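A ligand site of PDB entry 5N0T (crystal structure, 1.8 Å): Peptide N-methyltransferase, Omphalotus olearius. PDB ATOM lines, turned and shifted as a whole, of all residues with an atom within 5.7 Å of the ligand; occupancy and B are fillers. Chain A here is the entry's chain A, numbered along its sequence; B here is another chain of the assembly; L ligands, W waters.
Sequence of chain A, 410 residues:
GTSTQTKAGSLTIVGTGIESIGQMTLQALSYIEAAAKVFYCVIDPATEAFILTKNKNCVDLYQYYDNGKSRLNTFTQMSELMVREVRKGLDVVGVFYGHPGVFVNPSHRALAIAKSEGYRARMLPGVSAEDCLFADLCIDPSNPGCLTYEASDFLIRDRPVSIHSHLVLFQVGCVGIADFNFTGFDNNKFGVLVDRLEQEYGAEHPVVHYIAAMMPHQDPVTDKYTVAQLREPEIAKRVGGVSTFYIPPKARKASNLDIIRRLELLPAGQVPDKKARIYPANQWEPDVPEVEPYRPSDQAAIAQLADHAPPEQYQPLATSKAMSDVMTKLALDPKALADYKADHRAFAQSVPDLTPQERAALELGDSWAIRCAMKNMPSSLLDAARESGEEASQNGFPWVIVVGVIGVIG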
ATOM      1  N   ILE A  18     -18.335 -15.577   3.437  1.00  0.00           N
ATOM      2  CA  ILE A  18     -19.138 -14.436   3.858  1.00  0.00           C
ATOM      3  C   ILE A  18     -20.593 -14.576   3.458  1.00  0.00           C
ATOM      4  O   ILE A  18     -21.482 -14.406   4.305  1.00  0.00           O
ATOM      5  CB  ILE A  18     -18.573 -13.085   3.369  1.00  0.00           C
ATOM      6  CG1 ILE A  18     -17.171 -12.842   3.940  1.00  0.00           C
ATOM      7  CG2 ILE A  18     -19.516 -11.941   3.735  1.00  0.00           C
ATOM      8  CD1 ILE A  18     -17.050 -12.690   5.447  1.00  0.00           C
ATOM      9  N   ILE A  43     -22.720 -15.913  11.647  1.00  0.00           N
ATOM     10  CA  ILE A  43     -23.612 -14.774  11.923  1.00  0.00           C
ATOM     11  C   ILE A  43     -24.901 -14.753  11.102  1.00  0.00           C
ATOM     12  O   ILE A  43     -25.628 -13.750  11.149  1.00  0.00           O
ATOM     13  CB  ILE A  43     -22.887 -13.411  11.916  1.00  0.00           C
ATOM     14  CG1 ILE A  43     -22.202 -13.129  10.588  1.00  0.00           C
ATOM     15  CG2 ILE A  43     -21.893 -13.313  13.073  1.00  0.00           C
ATOM     16  CD1 ILE A  43     -21.843 -11.656  10.463  1.00  0.00           C
ATOM     17  N   TYR A  97     -16.959 -17.789  10.743  1.00  0.00           N
ATOM     18  CA  TYR A  97     -17.384 -16.902   9.629  1.00  0.00           C
ATOM     19  C   TYR A  97     -16.184 -16.453   8.778  1.00  0.00           C
ATOM     20  O   TYR A  97     -15.127 -16.136   9.322  1.00  0.00           O
ATOM     21  CB  TYR A  97     -18.118 -15.684  10.270  1.00  0.00           C
ATOM     22  CG  TYR A  97     -18.690 -14.574   9.390  1.00  0.00           C
ATOM     23  CD1 TYR A  97     -19.622 -14.829   8.381  1.00  0.00           C
ATOM     24  CD2 TYR A  97     -18.334 -13.233   9.632  1.00  0.00           C
ATOM     25  CE1 TYR A  97     -20.164 -13.781   7.616  1.00  0.00           C
ATOM     26  CE2 TYR A  97     -18.860 -12.197   8.872  1.00  0.00           C
ATOM     27  CZ  TYR A  97     -19.760 -12.448   7.853  1.00  0.00           C
ATOM     28  OH  TYR A  97     -20.300 -11.362   7.140  1.00  0.00           O
ATOM     29  N   GLY A  98     -16.312 -16.462   7.446  1.00  0.00           N
ATOM     30  CA  GLY A  98     -15.272 -15.903   6.584  1.00  0.00           C
ATOM     31  C   GLY A  98     -14.052 -16.813   6.452  1.00  0.00           C
ATOM     32  O   GLY A  98     -14.197 -18.011   6.169  1.00  0.00           O
ATOM     33  N   HIS A  99     -12.875 -16.229   6.652  1.00  0.00           N
ATOM     34  CA  HIS A  99     -11.594 -16.940   6.788  1.00  0.00           C
ATOM     35  C   HIS A  99     -11.368 -17.032   8.300  1.00  0.00           C
ATOM     36  O   HIS A  99     -11.448 -16.001   9.006  1.00  0.00           O
ATOM     37  CB  HIS A  99     -10.476 -16.142   6.127  1.00  0.00           C
ATOM     38  CG  HIS A  99      -9.104 -16.778   6.133  1.00  0.00           C
ATOM     39  ND1 HIS A  99      -8.488 -17.229   7.271  1.00  0.00           N
ATOM     40  CD2 HIS A  99      -8.199 -16.925   5.133  1.00  0.00           C
ATOM     41  CE1 HIS A  99      -7.279 -17.663   6.981  1.00  0.00           C
ATOM     42  NE2 HIS A  99      -7.069 -17.476   5.681  1.00  0.00           N
ATOM     43  N   PRO A 100     -11.130 -18.254   8.823  1.00  0.00           N
ATOM     44  CA  PRO A 100     -11.107 -18.386  10.282  1.00  0.00           C
ATOM     45  C   PRO A 100      -9.904 -17.807  11.037  1.00  0.00           C
ATOM     46  O   PRO A 100      -9.898 -17.838  12.278  1.00  0.00           O
ATOM     47  CB  PRO A 100     -11.184 -19.896  10.477  1.00  0.00           C
ATOM     48  CG  PRO A 100     -10.517 -20.451   9.259  1.00  0.00           C
ATOM     49  CD  PRO A 100     -10.863 -19.519   8.138  1.00  0.00           C
ATOM     50  N   VAL A 102      -8.604 -14.553   9.917  1.00  0.00           N
ATOM     51  CA  VAL A 102      -8.581 -13.140   9.485  1.00  0.00           C
ATOM     52  C   VAL A 102      -9.528 -12.360  10.411  1.00  0.00           C
ATOM     53  O   VAL A 102     -10.746 -12.556  10.370  1.00  0.00           O
ATOM     54  CB  VAL A 102      -9.004 -13.011   8.015  1.00  0.00           C
ATOM     55  CG1 VAL A 102      -9.243 -11.556   7.593  1.00  0.00           C
ATOM     56  CG2 VAL A 102      -7.955 -13.643   7.109  1.00  0.00           C
ATOM     57  N   PHE A 103      -8.943 -11.504  11.258  1.00  0.00           N
ATOM     58  CA  PHE A 103      -9.667 -10.771  12.319  1.00  0.00           C
ATOM     59  C   PHE A 103     -10.482 -11.701  13.236  1.00  0.00           C
ATOM     60  O   PHE A 103     -11.672 -11.468  13.451  1.00  0.00           O
ATOM     61  CB  PHE A 103     -10.538  -9.630  11.731  1.00  0.00           C
ATOM     62  CG  PHE A 103      -9.750  -8.520  11.065  1.00  0.00           C
ATOM     63  CD1 PHE A 103      -9.033  -8.754   9.890  1.00  0.00           C
ATOM     64  CD2 PHE A 103      -9.688  -7.246  11.624  1.00  0.00           C
ATOM     65  CE1 PHE A 103      -8.272  -7.743   9.301  1.00  0.00           C
ATOM     66  CE2 PHE A 103      -8.947  -6.244  11.028  1.00  0.00           C
ATOM     67  CZ  PHE A 103      -8.220  -6.490   9.878  1.00  0.00           C
ATOM     68  N   VAL A 104      -9.827 -12.755  13.764  1.00  0.00           N
ATOM     69  CA  VAL A 104     -10.437 -13.725  14.685  1.00  0.00           C
ATOM     70  C   VAL A 104      -9.454 -14.007  15.822  1.00  0.00           C
ATOM     71  O   VAL A 104      -8.298 -14.254  15.555  1.00  0.00           O
ATOM     72  CB  VAL A 104     -10.763 -15.086  13.980  1.00  0.00           C
ATOM     73  CG1 VAL A 104     -11.407 -16.066  14.942  1.00  0.00           C
ATOM     74  CG2 VAL A 104     -11.652 -14.883  12.769  1.00  0.00           C
ATOM     75  N   VAL A 127     -12.753 -17.738   2.365  1.00  0.00           N
ATOM     76  CA  VAL A 127     -13.009 -16.430   1.750  1.00  0.00           C
ATOM     77  C   VAL A 127     -13.325 -15.351   2.800  1.00  0.00           C
ATOM     78  O   VAL A 127     -14.319 -15.448   3.544  1.00  0.00           O
ATOM     79  CB  VAL A 127     -14.196 -16.542   0.732  1.00  0.00           C
ATOM     80  CG1 VAL A 127     -14.662 -15.188   0.218  1.00  0.00           C
ATOM     81  CG2 VAL A 127     -13.799 -17.453  -0.431  1.00  0.00           C
ATOM     82  N   SER A 128     -12.476 -14.318   2.890  1.00  0.00           N
ATOM     83  CA  SER A 128     -12.681 -13.211   3.838  1.00  0.00           C
ATOM     84  C   SER A 128     -13.518 -12.065   3.282  1.00  0.00           C
ATOM     85  O   SER A 128     -13.791 -11.978   2.060  1.00  0.00           O
ATOM     86  CB  SER A 128     -11.305 -12.631   4.239  1.00  0.00           C
ATOM     87  OG  SER A 128     -10.765 -11.876   3.152  1.00  0.00           O
ATOM     88  N   ALA A 129     -13.879 -11.135   4.183  1.00  0.00           N
ATOM     89  CA  ALA A 129     -14.521  -9.888   3.772  1.00  0.00           C
ATOM     90  C   ALA A 129     -13.641  -9.038   2.824  1.00  0.00           C
ATOM     91  O   ALA A 129     -14.185  -8.367   1.937  1.00  0.00           O
ATOM     92  CB  ALA A 129     -14.958  -9.058   4.975  1.00  0.00           C
ATOM     93  N   GLU A 130     -12.315  -9.080   2.996  1.00  0.00           N
ATOM     94  CA  GLU A 130     -11.405  -8.397   2.071  1.00  0.00           C
ATOM     95  C   GLU A 130     -11.414  -9.051   0.670  1.00  0.00           C
ATOM     96  O   GLU A 130     -11.430  -8.341  -0.343  1.00  0.00           O
ATOM     97  CB  GLU A 130      -9.982  -8.286   2.650  1.00  0.00           C
ATOM     98  CG  GLU A 130      -9.005  -7.566   1.735  1.00  0.00           C
ATOM     99  CD  GLU A 130      -7.717  -7.138   2.425  1.00  0.00           C
ATOM    100  OE1 GLU A 130      -6.718  -7.895   2.408  1.00  0.00           O
ATOM    101  OE2 GLU A 130      -7.697  -6.024   2.993  1.00  0.00           O
ATOM    102  N   LEU A 169      -9.923  -0.657   5.947  1.00  0.00           N
ATOM    103  CA  LEU A 169     -10.109  -0.592   7.398  1.00  0.00           C
ATOM    104  C   LEU A 169     -11.323  -1.433   7.840  1.00  0.00           C
ATOM    105  O   LEU A 169     -12.439  -1.152   7.427  1.00  0.00           O
ATOM    106  CB  LEU A 169     -10.314   0.846   7.838  1.00  0.00           C
ATOM    107  CG  LEU A 169      -9.170   1.832   7.603  1.00  0.00           C
ATOM    108  CD1 LEU A 169      -9.558   3.217   8.100  1.00  0.00           C
ATOM    109  CD2 LEU A 169      -7.886   1.391   8.282  1.00  0.00           C
ATOM    110  N   PHE A 170     -11.078  -2.454   8.678  1.00  0.00           N
ATOM    111  CA  PHE A 170     -12.133  -3.276   9.297  1.00  0.00           C
ATOM    112  C   PHE A 170     -12.571  -2.667  10.639  1.00  0.00           C
ATOM    113  O   PHE A 170     -11.807  -1.923  11.273  1.00  0.00           O
ATOM    114  CB  PHE A 170     -11.627  -4.676   9.656  1.00  0.00           C
ATOM    115  CG  PHE A 170     -11.501  -5.660   8.481  1.00  0.00           C
ATOM    116  CD1 PHE A 170     -10.747  -5.361   7.353  1.00  0.00           C
ATOM    117  CD2 PHE A 170     -12.074  -6.931   8.588  1.00  0.00           C
ATOM    118  CE1 PHE A 170     -10.596  -6.307   6.322  1.00  0.00           C
ATOM    119  CE2 PHE A 170     -11.936  -7.884   7.574  1.00  0.00           C
ATOM    120  CZ  PHE A 170     -11.202  -7.566   6.429  1.00  0.00           C
ATOM    121  N   GLN A 171     -13.766  -3.043  11.092  1.00  0.00           N
ATOM    122  CA  GLN A 171     -14.278  -2.643  12.424  1.00  0.00           C
ATOM    123  C   GLN A 171     -14.412  -1.138  12.613  1.00  0.00           C
ATOM    124  O   GLN A 171     -14.241  -0.615  13.721  1.00  0.00           O
ATOM    125  CB  GLN A 171     -13.477  -3.314  13.582  1.00  0.00           C
ATOM    126  CG  GLN A 171     -13.525  -4.823  13.450  1.00  0.00           C
ATOM    127  CD  GLN A 171     -12.976  -5.636  14.614  1.00  0.00           C
ATOM    128  OE1 GLN A 171     -13.141  -6.853  14.588  1.00  0.00           O
ATOM    129  NE2 GLN A 171     -12.326  -5.023  15.590  1.00  0.00           N
ATOM    130  N   VAL A 172     -14.804  -0.437  11.543  1.00  0.00           N
ATOM    131  CA  VAL A 172     -15.063   1.012  11.609  1.00  0.00           C
ATOM    132  C   VAL A 172     -16.344   1.382  12.360  1.00  0.00           C
ATOM    133  O   VAL A 172     -16.521   2.557  12.749  1.00  0.00           O
ATOM    134  CB  VAL A 172     -15.079   1.660  10.199  1.00  0.00           C
ATOM    135  CG1 VAL A 172     -13.698   1.542   9.571  1.00  0.00           C
ATOM    136  CG2 VAL A 172     -16.142   1.010   9.290  1.00  0.00           C
ATOM    137  N   CSO A 174     -17.170   0.163  15.377  1.00  0.00           N
ATOM    138  CA  CSO A 174     -16.981   0.122  16.845  1.00  0.00           C
ATOM    139  CB  CSO A 174     -17.184  -1.315  17.357  1.00  0.00           C
ATOM    140  SG  CSO A 174     -16.207  -2.447  16.435  1.00  0.00           S
ATOM    141  C   CSO A 174     -15.651   0.664  17.285  1.00  0.00           C
ATOM    142  O   CSO A 174     -14.894   0.023  18.008  1.00  0.00           O
ATOM    143  OD  CSO A 174     -17.335  -2.921  15.188  1.00  0.00           O
ATOM    144  N   TYR A 210     -18.474  -0.137   2.490  1.00  0.00           N
ATOM    145  CA  TYR A 210     -18.650  -1.455   1.885  1.00  0.00           C
ATOM    146  C   TYR A 210     -19.291  -2.471   2.828  1.00  0.00           C
ATOM    147  O   TYR A 210     -18.787  -2.716   3.927  1.00  0.00           O
ATOM    148  CB  TYR A 210     -17.312  -2.000   1.375  1.00  0.00           C
ATOM    149  CG  TYR A 210     -17.438  -3.403   0.808  1.00  0.00           C
ATOM    150  CD1 TYR A 210     -18.196  -3.630  -0.334  1.00  0.00           C
ATOM    151  CD2 TYR A 210     -16.864  -4.510   1.448  1.00  0.00           C
ATOM    152  CE1 TYR A 210     -18.350  -4.920  -0.859  1.00  0.00           C
ATOM    153  CE2 TYR A 210     -17.001  -5.799   0.917  1.00  0.00           C
ATOM    154  CZ  TYR A 210     -17.759  -5.998  -0.236  1.00  0.00           C
ATOM    155  OH  TYR A 210     -17.904  -7.261  -0.801  1.00  0.00           O
ATOM    156  N   ILE A 211     -20.378  -3.101   2.363  1.00  0.00           N
ATOM    157  CA  ILE A 211     -20.950  -4.263   3.056  1.00  0.00           C
ATOM    158  C   ILE A 211     -21.252  -5.367   2.030  1.00  0.00           C
ATOM    159  O   ILE A 211     -22.135  -5.174   1.178  1.00  0.00           O
ATOM    160  CB  ILE A 211     -22.259  -3.938   3.820  1.00  0.00           C
ATOM    161  CG1 ILE A 211     -22.065  -2.737   4.769  1.00  0.00           C
ATOM    162  CG2 ILE A 211     -22.706  -5.175   4.596  1.00  0.00           C
ATOM    163  CD1 ILE A 211     -23.348  -2.279   5.423  1.00  0.00           C
ATOM    164  N   ALA A 212     -20.519  -6.478   2.101  1.00  0.00           N
ATOM    165  CA  ALA A 212     -20.764  -7.624   1.240  1.00  0.00           C
ATOM    166  C   ALA A 212     -22.149  -8.178   1.540  1.00  0.00           C
ATOM    167  O   ALA A 212     -22.580  -8.205   2.694  1.00  0.00           O
ATOM    168  CB  ALA A 212     -19.734  -8.729   1.479  1.00  0.00           C
ATOM    169  N   ALA A 213     -22.829  -8.627   0.499  1.00  0.00           N
ATOM    170  CA  ALA A 213     -24.101  -9.341   0.626  1.00  0.00           C
ATOM    171  C   ALA A 213     -23.910 -10.624   1.461  1.00  0.00           C
ATOM    172  O   ALA A 213     -23.000 -11.419   1.175  1.00  0.00           O
ATOM    173  CB  ALA A 213     -24.611  -9.701  -0.750  1.00  0.00           C
ATOM    174  N   MET A 214     -24.735 -10.809   2.481  1.00  0.00           N
ATOM    175  CA  MET A 214     -24.670 -12.014   3.326  1.00  0.00           C
ATOM    176  C   MET A 214     -25.675 -13.095   2.904  1.00  0.00           C
ATOM    177  O   MET A 214     -25.481 -14.262   3.213  1.00  0.00           O
ATOM    178  CB  MET A 214     -24.801 -11.641   4.812  1.00  0.00           C
ATOM    179  CG  MET A 214     -23.495 -11.102   5.401  1.00  0.00           C
ATOM    180  SD  MET A 214     -23.661 -10.113   6.909  1.00  0.00           S
ATOM    181  CE  MET A 214     -24.496  -8.640   6.308  1.00  0.00           C
ATOM    182  N   GLY A 240     -22.208   0.193  10.594  1.00  0.00           N
ATOM    183  CA  GLY A 240     -22.559  -0.815  11.609  1.00  0.00           C
ATOM    184  C   GLY A 240     -21.489  -1.875  11.798  1.00  0.00           C
ATOM    185  O   GLY A 240     -20.329  -1.714  11.400  1.00  0.00           O
ATOM    186  N   GLY A 241     -21.892  -2.980  12.408  1.00  0.00           N
ATOM    187  CA  GLY A 241     -20.958  -4.015  12.826  1.00  0.00           C
ATOM    188  C   GLY A 241     -20.367  -4.872  11.735  1.00  0.00           C
ATOM    189  O   GLY A 241     -19.335  -5.507  11.969  1.00  0.00           O
ATOM    190  N   VAL A 242     -20.989  -4.887  10.549  1.00  0.00           N
ATOM    191  CA  VAL A 242     -20.409  -5.578   9.379  1.00  0.00           C
ATOM    192  C   VAL A 242     -19.902  -4.614   8.268  1.00  0.00           C
ATOM    193  O   VAL A 242     -19.777  -5.014   7.096  1.00  0.00           O
ATOM    194  CB  VAL A 242     -21.379  -6.635   8.789  1.00  0.00           C
ATOM    195  CG1 VAL A 242     -21.488  -7.803   9.768  1.00  0.00           C
ATOM    196  CG2 VAL A 242     -22.734  -6.041   8.463  1.00  0.00           C
ATOM    197  N   SER A 243     -19.590  -3.376   8.666  1.00  0.00           N
ATOM    198  CA  SER A 243     -19.113  -2.321   7.754  1.00  0.00           C
ATOM    199  C   SER A 243     -17.571  -2.329   7.681  1.00  0.00           C
ATOM    200  O   SER A 243     -16.901  -2.430   8.716  1.00  0.00           O
ATOM    201  CB  SER A 243     -19.572  -0.937   8.261  1.00  0.00           C
ATOM    202  OG  SER A 243     -20.975  -0.743   8.177  1.00  0.00           O
ATOM    203  N   THR A 244     -17.050  -2.203   6.460  1.00  0.00           N
ATOM    204  CA  THR A 244     -15.616  -2.020   6.181  1.00  0.00           C
ATOM    205  C   THR A 244     -15.478  -0.750   5.326  1.00  0.00           C
ATOM    206  O   THR A 244     -16.370  -0.440   4.553  1.00  0.00           O
ATOM    207  CB  THR A 244     -15.077  -3.291   5.468  1.00  0.00           C
ATOM    208  OG1 THR A 244     -15.137  -4.406   6.388  1.00  0.00           O
ATOM    209  CG2 THR A 244     -13.645  -3.133   4.968  1.00  0.00           C
ATOM    210  N   VAL B 400     -19.654  -9.638  16.585  1.00  0.00           N
ATOM    211  CA  VAL B 400     -18.393 -10.330  16.872  1.00  0.00           C
ATOM    212  C   VAL B 400     -17.269  -9.415  16.400  1.00  0.00           C
ATOM    213  O   VAL B 400     -17.369  -8.839  15.310  1.00  0.00           O
ATOM    214  CB  VAL B 400     -18.360 -11.674  16.134  1.00  0.00           C
ATOM    215  CG1 VAL B 400     -16.989 -12.327  16.224  1.00  0.00           C
ATOM    216  CG2 VAL B 400     -19.436 -12.602  16.674  1.00  0.00           C
ATOM    217  N   ILE B 401     -16.215  -9.256  17.207  1.00  0.00           N
ATOM    218  CA  ILE B 401     -15.021  -8.456  16.843  1.00  0.00           C
ATOM    219  C   ILE B 401     -13.704  -9.128  17.253  1.00  0.00           C
ATOM    220  O   ILE B 401     -13.655  -9.990  18.151  1.00  0.00           O
ATOM    221  CB  ILE B 401     -15.052  -7.039  17.476  1.00  0.00           C
ATOM    222  CG1 ILE B 401     -15.101  -7.105  18.994  1.00  0.00           C
ATOM    223  CG2 ILE B 401     -16.245  -6.244  16.957  1.00  0.00           C
ATOM    224  CD1 ILE B 401     -14.967  -5.773  19.680  1.00  0.00           C
ATOM    225  N   VAL B 402     -12.611  -8.718  16.589  1.00  0.00           N
ATOM    226  CA  VAL B 402     -11.275  -9.080  17.021  1.00  0.00           C
ATOM    227  C   VAL B 402     -10.834  -8.018  18.051  1.00  0.00           C
ATOM    228  O   VAL B 402     -11.139  -6.827  17.895  1.00  0.00           O
ATOM    229  CB  VAL B 402     -10.269  -9.189  15.853  1.00  0.00           C
ATOM    230  CG1 VAL B 402      -9.803  -7.822  15.343  1.00  0.00           C
ATOM    231  CG2 VAL B 402      -9.050 -10.007  16.275  1.00  0.00           C
HETATM  232  N1  LIG L   1     -13.235 -13.645   9.726  1.00  0.00           N
HETATM  233  C1  LIG L   1     -13.976 -12.533   9.116  1.00  0.00           C
HETATM  234  C2  LIG L   1     -13.469 -12.425   7.691  1.00  0.00           C
HETATM  235  O1  LIG L   1     -13.663 -11.369   7.027  1.00  0.00           O
HETATM  236  O2  LIG L   1     -12.874 -13.408   7.202  1.00  0.00           O
HETATM  237  C3  LIG L   1     -13.817 -11.148   9.820  1.00  0.00           C
HETATM  238  C4  LIG L   1     -14.368 -11.060  11.260  1.00  0.00           C
HETATM  239  S1  LIG L   1     -14.206  -9.568  12.100  1.00  0.00           S
HETATM  240  C5  LIG L   1     -14.326 -10.030  13.695  1.00  0.00           C
HETATM  241  C6  LIG L   1     -15.461  -8.460  11.862  1.00  0.00           C
HETATM  242  C7  LIG L   1     -15.220  -7.396  10.791  1.00  0.00           C
HETATM  243  O3  LIG L   1     -15.134  -7.992   9.493  1.00  0.00           O
HETATM  244  C8  LIG L   1     -16.317  -6.359  10.625  1.00  0.00           C
HETATM  245  O4  LIG L   1     -16.253  -5.239  11.523  1.00  0.00           O
HETATM  246  C9  LIG L   1     -16.096  -5.885   9.199  1.00  0.00           C
HETATM  247  O5  LIG L   1     -15.040  -4.922   9.135  1.00  0.00           O
HETATM  248  C10 LIG L   1     -15.692  -7.151   8.463  1.00  0.00           C
HETATM  249  N2  LIG L   1     -16.909  -7.739   7.851  1.00  0.00           N
HETATM  250  C11 LIG L   1     -17.633  -8.788   8.316  1.00  0.00           C
HETATM  251  N3  LIG L   1     -18.716  -9.041   7.521  1.00  0.00           N
HETATM  252  C12 LIG L   1     -18.671  -8.146   6.505  1.00  0.00           C
HETATM  253  C13 LIG L   1     -19.511  -7.836   5.329  1.00  0.00           C
HETATM  254  N4  LIG L   1     -20.628  -8.568   5.024  1.00  0.00           N
HETATM  255  N5  LIG L   1     -19.113  -6.826   4.540  1.00  0.00           N
HETATM  256  C14 LIG L   1     -17.998  -6.082   4.802  1.00  0.00           C
HETATM  257  N6  LIG L   1     -17.211  -6.282   5.886  1.00  0.00           N
HETATM  258  C15 LIG L   1     -17.497  -7.290   6.743  1.00  0.00           C
HETATM  259  O   HOH W   1     -17.622  -2.370  11.288  1.00  0.00           O
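The backbone NH (N) of His 99 lies within hydrogen-bond range of an oxygen (O2) of the ligand (2.9 Å).
A nitrogen (N5) of the ligand sits at hydrogen-bond distance from the backbone NH (N) of Ala 212, 2.8 Å away.
An oxygen (O5) of the ligand is in hydrogen-bond range of the backbone carbonyl oxygen (O) of Ser 243, at 3.1 Å.
The side-chain hydroxyl (OG1) of Thr 244 is in hydrogen-bond range of an oxygen (O5) of the ligand.
N1 of the ligand lies within hydrogen-bond range of O of His 99 (3.0 Å).
The backbone carbonyl oxygen (O) of Gly 241 is in hydrogen-bond range of an oxygen (O4) of the ligand, 3.1 Å away.
The backbone NH of Gln 171 sits at hydrogen-bond distance from an oxygen (O5) of the ligand (3.0 Å).
O of Val 102 lies within hydrogen-bond range of N1 of the ligand (2.8 Å).
The backbone carbonyl oxygen of Ala 212 lies within hydrogen-bond range of a nitrogen (N4) of the ligand (3.1 Å).
O1 of the ligand lies within hydrogen-bond range of N of Ala 129.
O of Tyr 97 lies within hydrogen-bond range of N1 of the ligand (3.2 Å).
A nitrogen (N3) of the ligand is in hydrogen-bond range of the side-chain hydroxyl of Tyr 97, at 2.8 Å.
The side-chain amide oxygen (OE1) of Gln 171 lies within hydrogen-bond range of the backbone NH (N) of Val 402 of chain B (2.8 Å).
The side-chain sulfur (SD) of Met 214 lies within hydrogen-bond range of the side-chain hydroxyl (OH) of Tyr 97.
OG of Ser 243 lies within hydrogen-bond range of N of Gly 240, at 2.9 Å.
OG of Ser 128 is in hydrogen-bond range of N of Glu 130.
The backbone carbonyl oxygen (O) of Thr 244 lies within hydrogen-bond range of the backbone NH (N) of Tyr 210.
O of Phe 103 lies close to S1 of the ligand (3.4 Å).
A nitrogen (N6) of the ligand sits close to the backbone carbonyl oxygen (O) of Val 242 (3.1 Å).
Merely in contact with the ligand: Ile 18 (3.8 Å), Gly 98 (3.5 Å), Val 104 (3.6 Å), Ser 128 (3.4 Å), Phe 170 (3.3 Å), Tyr 210 (3.6 Å), Ile 211 (3.5 Å), Met 214 (3.8 Å), Val 400 of chain B (3.6 Å), Ile 401 of chain B (3.6 Å) and Val 402 of chain B (3.6 Å).
Hydrophobic or aromatic side chains that line the ligand: Ile 18, Tyr 97, His 99, Val 102, Phe 103, Val 104, Ala 129, Phe 170, Tyr 210, Ile 211, Ala 212, Met 214 and Val 242.
Within 4 Å of the ligand: Ile 18, Tyr 97, Gly 98, His 99, Val 102, Phe 103, Val 104, Ser 128, Ala 129, Phe 170, Gln 171, Tyr 210, Ile 211, Ala 212, Met 214, Gly 241, Val 242, Ser 243, Thr 244, Val 400 of chain B, Ile 401 of chain B and Val 402 of chain B.
Water W1 lies within hydrogen-bond range of the backbone carbonyl oxygen of Ser 243, the backbone carbonyl oxygen of Gly 240, an oxygen (O4) of the ligand and the backbone NH of Val 172.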
